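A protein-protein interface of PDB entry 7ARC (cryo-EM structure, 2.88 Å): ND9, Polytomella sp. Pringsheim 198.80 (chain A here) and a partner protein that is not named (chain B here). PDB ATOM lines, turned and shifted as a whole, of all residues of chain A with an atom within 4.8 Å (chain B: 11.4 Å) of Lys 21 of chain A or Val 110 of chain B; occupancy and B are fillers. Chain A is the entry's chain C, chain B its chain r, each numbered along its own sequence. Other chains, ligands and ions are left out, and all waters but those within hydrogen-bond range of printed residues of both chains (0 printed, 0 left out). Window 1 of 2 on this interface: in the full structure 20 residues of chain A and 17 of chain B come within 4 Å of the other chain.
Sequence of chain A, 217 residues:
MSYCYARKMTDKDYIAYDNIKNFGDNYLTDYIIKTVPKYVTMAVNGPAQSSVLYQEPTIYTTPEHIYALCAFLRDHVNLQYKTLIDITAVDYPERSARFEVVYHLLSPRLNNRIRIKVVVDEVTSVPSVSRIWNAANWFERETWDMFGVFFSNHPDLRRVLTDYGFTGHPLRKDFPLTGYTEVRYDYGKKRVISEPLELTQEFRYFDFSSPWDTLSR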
ATOM      1  N   TYR A  14       8.331   9.880  32.780  1.00  0.00           N
ATOM      2  CA  TYR A  14       7.628  11.057  32.295  1.00  0.00           C
ATOM      3  C   TYR A  14       6.652  10.695  31.182  1.00  0.00           C
ATOM      4  O   TYR A  14       6.924   9.824  30.351  1.00  0.00           O
ATOM      5  CB  TYR A  14       8.633  12.088  31.794  1.00  0.00           C
ATOM      6  CG  TYR A  14       9.522  11.592  30.676  1.00  0.00           C
ATOM      7  CD1 TYR A  14      10.767  11.041  30.945  1.00  0.00           C
ATOM      8  CD2 TYR A  14       9.130  11.703  29.349  1.00  0.00           C
ATOM      9  CE1 TYR A  14      11.584  10.595  29.927  1.00  0.00           C
ATOM     10  CE2 TYR A  14       9.940  11.260  28.326  1.00  0.00           C
ATOM     11  CZ  TYR A  14      11.167  10.710  28.619  1.00  0.00           C
ATOM     12  OH  TYR A  14      11.978  10.268  27.598  1.00  0.00           O
ATOM     13  N   ILE A  15       5.497  11.363  31.178  1.00  0.00           N
ATOM     14  CA  ILE A  15       4.571  11.211  30.062  1.00  0.00           C
ATOM     15  C   ILE A  15       5.141  11.858  28.802  1.00  0.00           C
ATOM     16  O   ILE A  15       5.001  11.320  27.697  1.00  0.00           O
ATOM     17  CB  ILE A  15       3.184  11.767  30.439  1.00  0.00           C
ATOM     18  CG1 ILE A  15       2.144  11.383  29.393  1.00  0.00           C
ATOM     19  CG2 ILE A  15       3.207  13.276  30.618  1.00  0.00           C
ATOM     20  CD1 ILE A  15       0.725  11.610  29.854  1.00  0.00           C
ATOM     21  N   ALA A  16       5.798  13.012  28.948  1.00  0.00           N
ATOM     22  CA  ALA A  16       6.548  13.693  27.894  1.00  0.00           C
ATOM     23  C   ALA A  16       7.206  14.923  28.510  1.00  0.00           C
ATOM     24  O   ALA A  16       6.973  15.258  29.674  1.00  0.00           O
ATOM     25  CB  ALA A  16       5.679  14.099  26.708  1.00  0.00           C
ATOM     26  N   TYR A  17       8.027  15.597  27.706  1.00  0.00           N
ATOM     27  CA  TYR A  17       8.713  16.801  28.153  1.00  0.00           C
ATOM     28  C   TYR A  17       7.746  17.978  28.241  1.00  0.00           C
ATOM     29  O   TYR A  17       6.684  17.992  27.615  1.00  0.00           O
ATOM     30  CB  TYR A  17       9.871  17.143  27.212  1.00  0.00           C
ATOM     31  CG  TYR A  17      11.043  16.191  27.294  1.00  0.00           C
ATOM     32  CD1 TYR A  17      11.165  15.292  28.345  1.00  0.00           C
ATOM     33  CD2 TYR A  17      12.035  16.197  26.322  1.00  0.00           C
ATOM     34  CE1 TYR A  17      12.239  14.424  28.424  1.00  0.00           C
ATOM     35  CE2 TYR A  17      13.113  15.333  26.392  1.00  0.00           C
ATOM     36  CZ  TYR A  17      13.210  14.448  27.445  1.00  0.00           C
ATOM     37  OH  TYR A  17      14.280  13.587  27.520  1.00  0.00           O
ATOM     38  N   ASP A  18       8.135  18.984  29.030  1.00  0.00           N
ATOM     39  CA  ASP A  18       7.261  20.134  29.257  1.00  0.00           C
ATOM     40  C   ASP A  18       7.008  20.914  27.970  1.00  0.00           C
ATOM     41  O   ASP A  18       5.866  21.280  27.669  1.00  0.00           O
ATOM     42  CB  ASP A  18       7.845  21.043  30.343  1.00  0.00           C
ATOM     43  CG  ASP A  18       9.190  21.636  29.961  1.00  0.00           C
ATOM     44  OD1 ASP A  18       9.713  21.309  28.875  1.00  0.00           O
ATOM     45  OD2 ASP A  18       9.715  22.456  30.742  1.00  0.00           O
ATOM     46  N   ASN A  19       8.065  21.189  27.203  1.00  0.00           N
ATOM     47  CA  ASN A  19       7.916  22.001  25.999  1.00  0.00           C
ATOM     48  C   ASN A  19       7.061  21.290  24.957  1.00  0.00           C
ATOM     49  O   ASN A  19       6.226  21.920  24.296  1.00  0.00           O
ATOM     50  CB  ASN A  19       9.288  22.369  25.431  1.00  0.00           C
ATOM     51  CG  ASN A  19      10.203  21.173  25.285  1.00  0.00           C
ATOM     52  OD1 ASN A  19      10.485  20.471  26.253  1.00  0.00           O
ATOM     53  ND2 ASN A  19      10.686  20.945  24.071  1.00  0.00           N
ATOM     54  N   ILE A  20       7.268  19.984  24.787  1.00  0.00           N
ATOM     55  CA  ILE A  20       6.479  19.215  23.829  1.00  0.00           C
ATOM     56  C   ILE A  20       5.006  19.236  24.218  1.00  0.00           C
ATOM     57  O   ILE A  20       4.123  19.340  23.358  1.00  0.00           O
ATOM     58  CB  ILE A  20       7.023  17.779  23.727  1.00  0.00           C
ATOM     59  CG1 ILE A  20       8.489  17.800  23.291  1.00  0.00           C
ATOM     60  CG2 ILE A  20       6.194  16.957  22.759  1.00  0.00           C
ATOM     61  CD1 ILE A  20       8.709  18.431  21.938  1.00  0.00           C
ATOM     62  N   LYS A  21       4.713  19.134  25.517  1.00  0.00           N
ATOM     63  CA  LYS A  21       3.332  19.251  25.975  1.00  0.00           C
ATOM     64  C   LYS A  21       2.757  20.634  25.709  1.00  0.00           C
ATOM     65  O   LYS A  21       1.632  20.750  25.219  1.00  0.00           O
ATOM     66  CB  LYS A  21       3.225  18.890  27.458  1.00  0.00           C
ATOM     67  CG  LYS A  21       3.628  17.464  27.795  1.00  0.00           C
ATOM     68  CD  LYS A  21       2.569  16.480  27.275  1.00  0.00           C
ATOM     69  CE  LYS A  21       2.857  15.920  25.890  1.00  0.00           C
ATOM     70  NZ  LYS A  21       1.843  14.904  25.513  1.00  0.00           N
ATOM     71  N   ASN A  22       3.495  21.693  26.047  1.00  0.00           N
ATOM     72  CA  ASN A  22       2.971  23.044  25.846  1.00  0.00           C
ATOM     73  C   ASN A  22       2.667  23.301  24.375  1.00  0.00           C
ATOM     74  O   ASN A  22       1.579  23.787  24.022  1.00  0.00           O
ATOM     75  CB  ASN A  22       3.962  24.077  26.382  1.00  0.00           C
ATOM     76  CG  ASN A  22       4.173  23.959  27.877  1.00  0.00           C
ATOM     77  OD1 ASN A  22       3.820  22.952  28.488  1.00  0.00           O
ATOM     78  ND2 ASN A  22       4.755  24.992  28.475  1.00  0.00           N
ATOM     79  N   PHE A  23       3.611  22.951  23.498  1.00  0.00           N
ATOM     80  CA  PHE A  23       3.435  23.072  22.053  1.00  0.00           C
ATOM     81  C   PHE A  23       2.562  21.922  21.567  1.00  0.00           C
ATOM     82  O   PHE A  23       3.031  20.887  21.087  1.00  0.00           O
ATOM     83  CB  PHE A  23       4.778  23.086  21.338  1.00  0.00           C
ATOM     84  CG  PHE A  23       4.672  23.388  19.876  1.00  0.00           C
ATOM     85  CD1 PHE A  23       3.843  24.400  19.425  1.00  0.00           C
ATOM     86  CD2 PHE A  23       5.385  22.650  18.949  1.00  0.00           C
ATOM     87  CE1 PHE A  23       3.737  24.678  18.082  1.00  0.00           C
ATOM     88  CE2 PHE A  23       5.281  22.925  17.601  1.00  0.00           C
ATOM     89  CZ  PHE A  23       4.456  23.940  17.169  1.00  0.00           C
ATOM     90  N   GLY A  24       1.259  22.125  21.692  1.00  0.00           N
ATOM     91  CA  GLY A  24       0.280  21.103  21.400  1.00  0.00           C
ATOM     92  C   GLY A  24      -0.832  21.162  22.418  1.00  0.00           C
ATOM     93  O   GLY A  24      -1.971  20.772  22.140  1.00  0.00           O
ATOM     94  N   ASP A  25      -0.510  21.660  23.611  1.00  0.00           N
ATOM     95  CA  ASP A  25      -1.548  21.988  24.572  1.00  0.00           C
ATOM     96  C   ASP A  25      -2.196  23.319  24.238  1.00  0.00           C
ATOM     97  O   ASP A  25      -3.424  23.445  24.305  1.00  0.00           O
ATOM     98  CB  ASP A  25      -0.971  22.017  25.987  1.00  0.00           C
ATOM     99  CG  ASP A  25      -0.990  20.657  26.652  1.00  0.00           C
ATOM    100  OD1 ASP A  25      -1.020  19.640  25.928  1.00  0.00           O
ATOM    101  OD2 ASP A  25      -0.974  20.606  27.899  1.00  0.00           O
ATOM    102  N   TYR A  54      -6.790  17.243  29.099  1.00  0.00           N
ATOM    103  CA  TYR A  54      -6.188  18.111  28.088  1.00  0.00           C
ATOM    104  C   TYR A  54      -7.187  18.508  26.996  1.00  0.00           C
ATOM    105  O   TYR A  54      -8.397  18.301  27.118  1.00  0.00           O
ATOM    106  CB  TYR A  54      -4.975  17.417  27.473  1.00  0.00           C
ATOM    107  CG  TYR A  54      -3.931  16.968  28.468  1.00  0.00           C
ATOM    108  CD1 TYR A  54      -3.551  17.782  29.524  1.00  0.00           C
ATOM    109  CD2 TYR A  54      -3.332  15.720  28.357  1.00  0.00           C
ATOM    110  CE1 TYR A  54      -2.599  17.371  30.436  1.00  0.00           C
ATOM    111  CE2 TYR A  54      -2.383  15.301  29.262  1.00  0.00           C
ATOM    112  CZ  TYR A  54      -2.021  16.129  30.302  1.00  0.00           C
ATOM    113  OH  TYR A  54      -1.071  15.716  31.207  1.00  0.00           O
ATOM    114  N   LEU A 110       4.725  13.914  19.490  1.00  0.00           N
ATOM    115  CA  LEU A 110       4.010  14.918  20.263  1.00  0.00           C
ATOM    116  C   LEU A 110       3.090  14.315  21.310  1.00  0.00           C
ATOM    117  O   LEU A 110       2.616  15.055  22.178  1.00  0.00           O
ATOM    118  CB  LEU A 110       3.183  15.815  19.338  1.00  0.00           C
ATOM    119  CG  LEU A 110       3.877  16.959  18.598  1.00  0.00           C
ATOM    120  CD1 LEU A 110       2.859  17.740  17.788  1.00  0.00           C
ATOM    121  CD2 LEU A 110       4.609  17.872  19.561  1.00  0.00           C
ATOM    122  N   ASN A 111       2.841  13.003  21.260  1.00  0.00           N
ATOM    123  CA  ASN A 111       1.906  12.353  22.179  1.00  0.00           C
ATOM    124  C   ASN A 111       0.554  13.053  22.117  1.00  0.00           C
ATOM    125  O   ASN A 111      -0.089  13.313  23.133  1.00  0.00           O
ATOM    126  CB  ASN A 111       2.458  12.334  23.605  1.00  0.00           C
ATOM    127  CG  ASN A 111       1.746  11.340  24.493  1.00  0.00           C
ATOM    128  OD1 ASN A 111       1.452  11.626  25.651  1.00  0.00           O
ATOM    129  ND2 ASN A 111       1.465  10.163  23.957  1.00  0.00           N
ATOM    130  N   PHE B  91       3.347  34.294  14.410  1.00  0.00           N
ATOM    131  CA  PHE B  91       3.366  33.359  15.523  1.00  0.00           C
ATOM    132  C   PHE B  91       4.546  33.653  16.441  1.00  0.00           C
ATOM    133  O   PHE B  91       5.604  34.113  16.004  1.00  0.00           O
ATOM    134  CB  PHE B  91       3.442  31.922  15.005  1.00  0.00           C
ATOM    135  CG  PHE B  91       3.273  30.878  16.068  1.00  0.00           C
ATOM    136  CD1 PHE B  91       2.079  30.755  16.754  1.00  0.00           C
ATOM    137  CD2 PHE B  91       4.305  30.005  16.367  1.00  0.00           C
ATOM    138  CE1 PHE B  91       1.922  29.791  17.727  1.00  0.00           C
ATOM    139  CE2 PHE B  91       4.152  29.038  17.338  1.00  0.00           C
ATOM    140  CZ  PHE B  91       2.960  28.932  18.019  1.00  0.00           C
ATOM    141  N   LYS B  95       7.882  31.682  22.510  1.00  0.00           N
ATOM    142  CA  LYS B  95       7.203  30.819  23.471  1.00  0.00           C
ATOM    143  C   LYS B  95       7.573  29.354  23.269  1.00  0.00           C
ATOM    144  O   LYS B  95       7.768  28.615  24.241  1.00  0.00           O
ATOM    145  CB  LYS B  95       5.692  31.013  23.360  1.00  0.00           C
ATOM    146  CG  LYS B  95       5.256  32.467  23.408  1.00  0.00           C
ATOM    147  CD  LYS B  95       5.551  33.095  24.760  1.00  0.00           C
ATOM    148  CE  LYS B  95       4.628  32.548  25.834  1.00  0.00           C
ATOM    149  NZ  LYS B  95       3.352  33.312  25.911  1.00  0.00           N
ATOM    150  N   VAL B  96       7.661  28.911  22.014  1.00  0.00           N
ATOM    151  CA  VAL B  96       7.877  27.495  21.735  1.00  0.00           C
ATOM    152  C   VAL B  96       9.301  27.075  22.089  1.00  0.00           C
ATOM    153  O   VAL B  96       9.514  26.060  22.762  1.00  0.00           O
ATOM    154  CB  VAL B  96       7.551  27.187  20.262  1.00  0.00           C
ATOM    155  CG1 VAL B  96       7.923  25.750  19.923  1.00  0.00           C
ATOM    156  CG2 VAL B  96       6.081  27.444  19.978  1.00  0.00           C
ATOM    157  N   PHE B  97      10.298  27.840  21.640  1.00  0.00           N
ATOM    158  CA  PHE B  97      11.690  27.419  21.743  1.00  0.00           C
ATOM    159  C   PHE B  97      12.514  28.168  22.784  1.00  0.00           C
ATOM    160  O   PHE B  97      13.638  27.743  23.071  1.00  0.00           O
ATOM    161  CB  PHE B  97      12.371  27.550  20.374  1.00  0.00           C
ATOM    162  CG  PHE B  97      11.864  26.573  19.356  1.00  0.00           C
ATOM    163  CD1 PHE B  97      11.827  25.219  19.637  1.00  0.00           C
ATOM    164  CD2 PHE B  97      11.399  27.010  18.127  1.00  0.00           C
ATOM    165  CE1 PHE B  97      11.355  24.315  18.706  1.00  0.00           C
ATOM    166  CE2 PHE B  97      10.923  26.110  17.194  1.00  0.00           C
ATOM    167  CZ  PHE B  97      10.902  24.762  17.484  1.00  0.00           C
ATOM    168  N   SER B  99      11.630  28.353  25.953  1.00  0.00           N
ATOM    169  CA  SER B  99      11.525  27.454  27.093  1.00  0.00           C
ATOM    170  C   SER B  99      12.078  26.065  26.809  1.00  0.00           C
ATOM    171  O   SER B  99      12.088  25.222  27.711  1.00  0.00           O
ATOM    172  CB  SER B  99      10.063  27.345  27.540  1.00  0.00           C
ATOM    173  OG  SER B  99       9.272  26.717  26.546  1.00  0.00           O
ATOM    174  N   ALA B 100      12.527  25.803  25.586  1.00  0.00           N
ATOM    175  CA  ALA B 100      13.073  24.492  25.262  1.00  0.00           C
ATOM    176  C   ALA B 100      14.478  24.338  25.845  1.00  0.00           C
ATOM    177  O   ALA B 100      15.275  25.279  25.801  1.00  0.00           O
ATOM    178  CB  ALA B 100      13.114  24.287  23.751  1.00  0.00           C
ATOM    179  N   PRO B 101      14.794  23.171  26.403  1.00  0.00           N
ATOM    180  CA  PRO B 101      16.141  22.946  26.945  1.00  0.00           C
ATOM    181  C   PRO B 101      17.204  22.992  25.857  1.00  0.00           C
ATOM    182  O   PRO B 101      16.980  22.566  24.723  1.00  0.00           O
ATOM    183  CB  PRO B 101      16.042  21.551  27.571  1.00  0.00           C
ATOM    184  CG  PRO B 101      14.879  20.907  26.888  1.00  0.00           C
ATOM    185  CD  PRO B 101      13.912  22.014  26.626  1.00  0.00           C
ATOM    186  N   ASP B 106      18.872  21.038  31.730  1.00  0.00           N
ATOM    187  CA  ASP B 106      17.705  21.910  31.711  1.00  0.00           C
ATOM    188  C   ASP B 106      16.422  21.174  31.354  1.00  0.00           C
ATOM    189  O   ASP B 106      15.356  21.797  31.331  1.00  0.00           O
ATOM    190  CB  ASP B 106      17.922  23.054  30.717  1.00  0.00           C
ATOM    191  CG  ASP B 106      18.988  24.031  31.171  1.00  0.00           C
ATOM    192  OD1 ASP B 106      19.172  24.191  32.396  1.00  0.00           O
ATOM    193  OD2 ASP B 106      19.645  24.638  30.300  1.00  0.00           O
ATOM    194  N   VAL B 107      16.500  19.874  31.076  1.00  0.00           N
ATOM    195  CA  VAL B 107      15.326  19.116  30.667  1.00  0.00           C
ATOM    196  C   VAL B 107      14.333  19.038  31.818  1.00  0.00           C
ATOM    197  O   VAL B 107      14.687  18.669  32.945  1.00  0.00           O
ATOM    198  CB  VAL B 107      15.732  17.715  30.185  1.00  0.00           C
ATOM    199  CG1 VAL B 107      14.502  16.845  29.984  1.00  0.00           C
ATOM    200  CG2 VAL B 107      16.531  17.813  28.894  1.00  0.00           C
ATOM    201  N   LYS B 108      13.081  19.380  31.534  1.00  0.00           N
ATOM    202  CA  LYS B 108      11.990  19.273  32.488  1.00  0.00           C
ATOM    203  C   LYS B 108      10.970  18.292  31.936  1.00  0.00           C
ATOM    204  O   LYS B 108      10.734  18.245  30.724  1.00  0.00           O
ATOM    205  CB  LYS B 108      11.330  20.630  32.754  1.00  0.00           C
ATOM    206  CG  LYS B 108      12.204  21.620  33.505  1.00  0.00           C
ATOM    207  CD  LYS B 108      11.510  22.964  33.665  1.00  0.00           C
ATOM    208  CE  LYS B 108      10.352  22.882  34.646  1.00  0.00           C
ATOM    209  NZ  LYS B 108      10.811  22.639  36.040  1.00  0.00           N
ATOM    210  N   THR B 109      10.369  17.512  32.824  1.00  0.00           N
ATOM    211  CA  THR B 109       9.488  16.424  32.435  1.00  0.00           C
ATOM    212  C   THR B 109       8.127  16.571  33.099  1.00  0.00           C
ATOM    213  O   THR B 109       8.008  17.112  34.202  1.00  0.00           O
ATOM    214  CB  THR B 109      10.097  15.069  32.803  1.00  0.00           C
ATOM    215  OG1 THR B 109      10.415  15.047  34.199  1.00  0.00           O
ATOM    216  CG2 THR B 109      11.356  14.808  31.994  1.00  0.00           C
ATOM    217  N   VAL B 110       7.103  16.076  32.413  1.00  0.00           N
ATOM    218  CA  VAL B 110       5.739  16.051  32.927  1.00  0.00           C
ATOM    219  C   VAL B 110       5.459  14.644  33.432  1.00  0.00           C
ATOM    220  O   VAL B 110       5.568  13.671  32.677  1.00  0.00           O
ATOM    221  CB  VAL B 110       4.723  16.465  31.852  1.00  0.00           C
ATOM    222  CG1 VAL B 110       3.328  16.540  32.446  1.00  0.00           C
ATOM    223  CG2 VAL B 110       5.116  17.796  31.236  1.00  0.00           C
ATOM    224  N   ARG B 111       5.123  14.530  34.712  1.00  0.00           N
ATOM    225  CA  ARG B 111       4.864  13.231  35.311  1.00  0.00           C
ATOM    226  C   ARG B 111       3.505  12.697  34.874  1.00  0.00           C
ATOM    227  O   ARG B 111       2.579  13.459  34.581  1.00  0.00           O
ATOM    228  CB  ARG B 111       4.932  13.331  36.834  1.00  0.00           C
ATOM    229  CG  ARG B 111       5.155  12.011  37.545  1.00  0.00           C
ATOM    230  CD  ARG B 111       5.675  12.237  38.956  1.00  0.00           C
ATOM    231  NE  ARG B 111       4.612  12.330  39.951  1.00  0.00           N
ATOM    232  CZ  ARG B 111       3.737  11.373  40.233  1.00  0.00           C
ATOM    233  NH1 ARG B 111       3.789  10.187  39.647  1.00  0.00           N
ATOM    234  NH2 ARG B 111       2.793  11.607  41.139  1.00  0.00           N
ATOM    235  N   ILE B 112       3.399  11.371  34.821  1.00  0.00           N
ATOM    236  CA  ILE B 112       2.131  10.740  34.439  1.00  0.00           C
ATOM    237  C   ILE B 112       1.074  11.048  35.490  1.00  0.00           C
ATOM    238  O   ILE B 112       1.365  10.969  36.701  1.00  0.00           O
ATOM    239  CB  ILE B 112       2.306   9.221  34.267  1.00  0.00           C
ATOM    240  CG1 ILE B 112       3.229   8.901  33.093  1.00  0.00           C
ATOM    241  CG2 ILE B 112       0.969   8.535  34.096  1.00  0.00           C
ATOM    242  CD1 ILE B 112       3.731   7.469  33.095  1.00  0.00           C
ATOM    243  N   PRO B 113      -0.146  11.420  35.105  1.00  0.00           N
ATOM    244  CA  PRO B 113      -1.204  11.614  36.105  1.00  0.00           C
ATOM    245  C   PRO B 113      -1.536  10.292  36.782  1.00  0.00           C
ATOM    246  O   PRO B 113      -1.846   9.299  36.121  1.00  0.00           O
ATOM    247  CB  PRO B 113      -2.385  12.149  35.287  1.00  0.00           C
ATOM    248  CG  PRO B 113      -2.058  11.861  33.864  1.00  0.00           C
ATOM    249  CD  PRO B 113      -0.576  11.790  33.747  1.00  0.00           C
ATOM    250  N   GLU B 114      -1.467  10.286  38.115  1.00  0.00           N
ATOM    251  CA  GLU B 114      -1.645   9.038  38.848  1.00  0.00           C
ATOM    252  C   GLU B 114      -3.088   8.552  38.792  1.00  0.00           C
ATOM    253  O   GLU B 114      -3.349   7.392  38.456  1.00  0.00           O
ATOM    254  CB  GLU B 114      -1.205   9.217  40.299  1.00  0.00           C
ATOM    255  CG  GLU B 114       0.277   9.438  40.500  1.00  0.00           C
ATOM    256  CD  GLU B 114       0.629   9.613  41.964  1.00  0.00           C
ATOM    257  OE1 GLU B 114      -0.301   9.682  42.797  1.00  0.00           O
ATOM    258  OE2 GLU B 114       1.835   9.684  42.285  1.00  0.00           O
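The backbone carbonyl oxygen of Lys 108 of chain B sits at hydrogen-bond distance from the backbone NH of Asp 18 of chain A (3.2 Å).
The backbone carbonyl oxygen (O) of Val 110 of chain B lies within hydrogen-bond range of the backbone NH (N) of Ile 15 of chain A (2.8 Å).
The backbone NH (N) of Val 110 of chain B sits at hydrogen-bond distance from the backbone carbonyl oxygen (O) of Ala 16 of chain A.
Of the 15 printed residues of chain A, 8 touch a printed residue of chain B.
Hydrophobic or aromatic side chains of chain B that line the printed part of chain A: Val 96, Pro 101, Val 107, Val 110 and Ile 112.
Along chain B the printed residues that touch a printed residue of chain A span positions 96 to 112.
Among the printed residues, no Asp or Glu carboxylate lies within 4 Å of a Lys or Arg side-chain nitrogen of the other chain.
Thr 109 of chain B touches Tyr 14 of chain A.
O of Val 110 of chain B touches CA of Tyr 14 of chain A, at 3.4 Å.
N of Ile 15 of chain A touches CG1 of Ile 112 of chain B (3.9 Å).
CE1 of Tyr 17 of chain A touches CG1 of Val 107 of chain B (3.7 Å).
Lys 108 of chain B touches Tyr 17 of chain A (O to CA, 3.6 Å).
Tyr 17 of chain A touches Val 110 of chain B.
Asp 18 of chain A touches Val 110 of chain B.
OD1 of Asn 19 of chain A touches CD of Pro 101 of chain B, 3.8 Å away.
CG of Lys 21 of chain A touches CG2 of Val 110 of chain B, at 3.8 Å.
Val 96 of chain B touches Phe 23 of chain A.
OD1 of Asp 18 of chain A sits close to OD1 of Asn 19 of chain A.
The backbone carbonyl oxygen (O) of Asp 18 of chain A lies close to the side-chain amide oxygen (OD1) of Asn 22 of chain A, at 2.8 Å.
The side-chain amino group (NZ) of Lys 21 of chain A sits at hydrogen-bond distance from the backbone carbonyl oxygen (O) of Leu 110 of chain A (3.4 Å).
The side-chain amide oxygen (OD1) of Asn 111 of chain A lies close to the side-chain amino group (NZ) of Lys 21 of chain A (3.3 Å).
Lys 21 of chain A touches one residue of chain B.
Of chain A, only Tyr 14 (3.4 Å), Ile 15 (2.8 Å), Ala 16 (2.9 Å), Tyr 17 (3.95 Å), Asp 18 (3.7 Å) and Lys 21 (3.8 Å) come within 4 Å of Val 110 of chain B.
Asp 18 of chain A touches just these residues of chain B: Lys 108 and Val 110.
Of chain B, only Pro 101 comes within 4 Å of Asn 19 of chain A.
No residue of chain B comes within 4 Å of Asn 22 of chain A.
No residue of chain B comes within 4 Å of Gly 24 of chain A.
No residue of chain B comes within 4 Å of Asn 111 of chain A.
Of the printed residues of chain B, Phe 23 of chain A touches Val 96.
Of the printed residues of chain A, Pro 101 of chain B touches Asn 19 (3.8 Å).
The nearest residue of chain A that does not touch Val 110 of chain B is Tyr 54 of chain A (4.6 Å).
The nearest printed residue of chain B that does not touch Tyr 14 of chain A is Ile 112 of chain B (4.3 Å).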
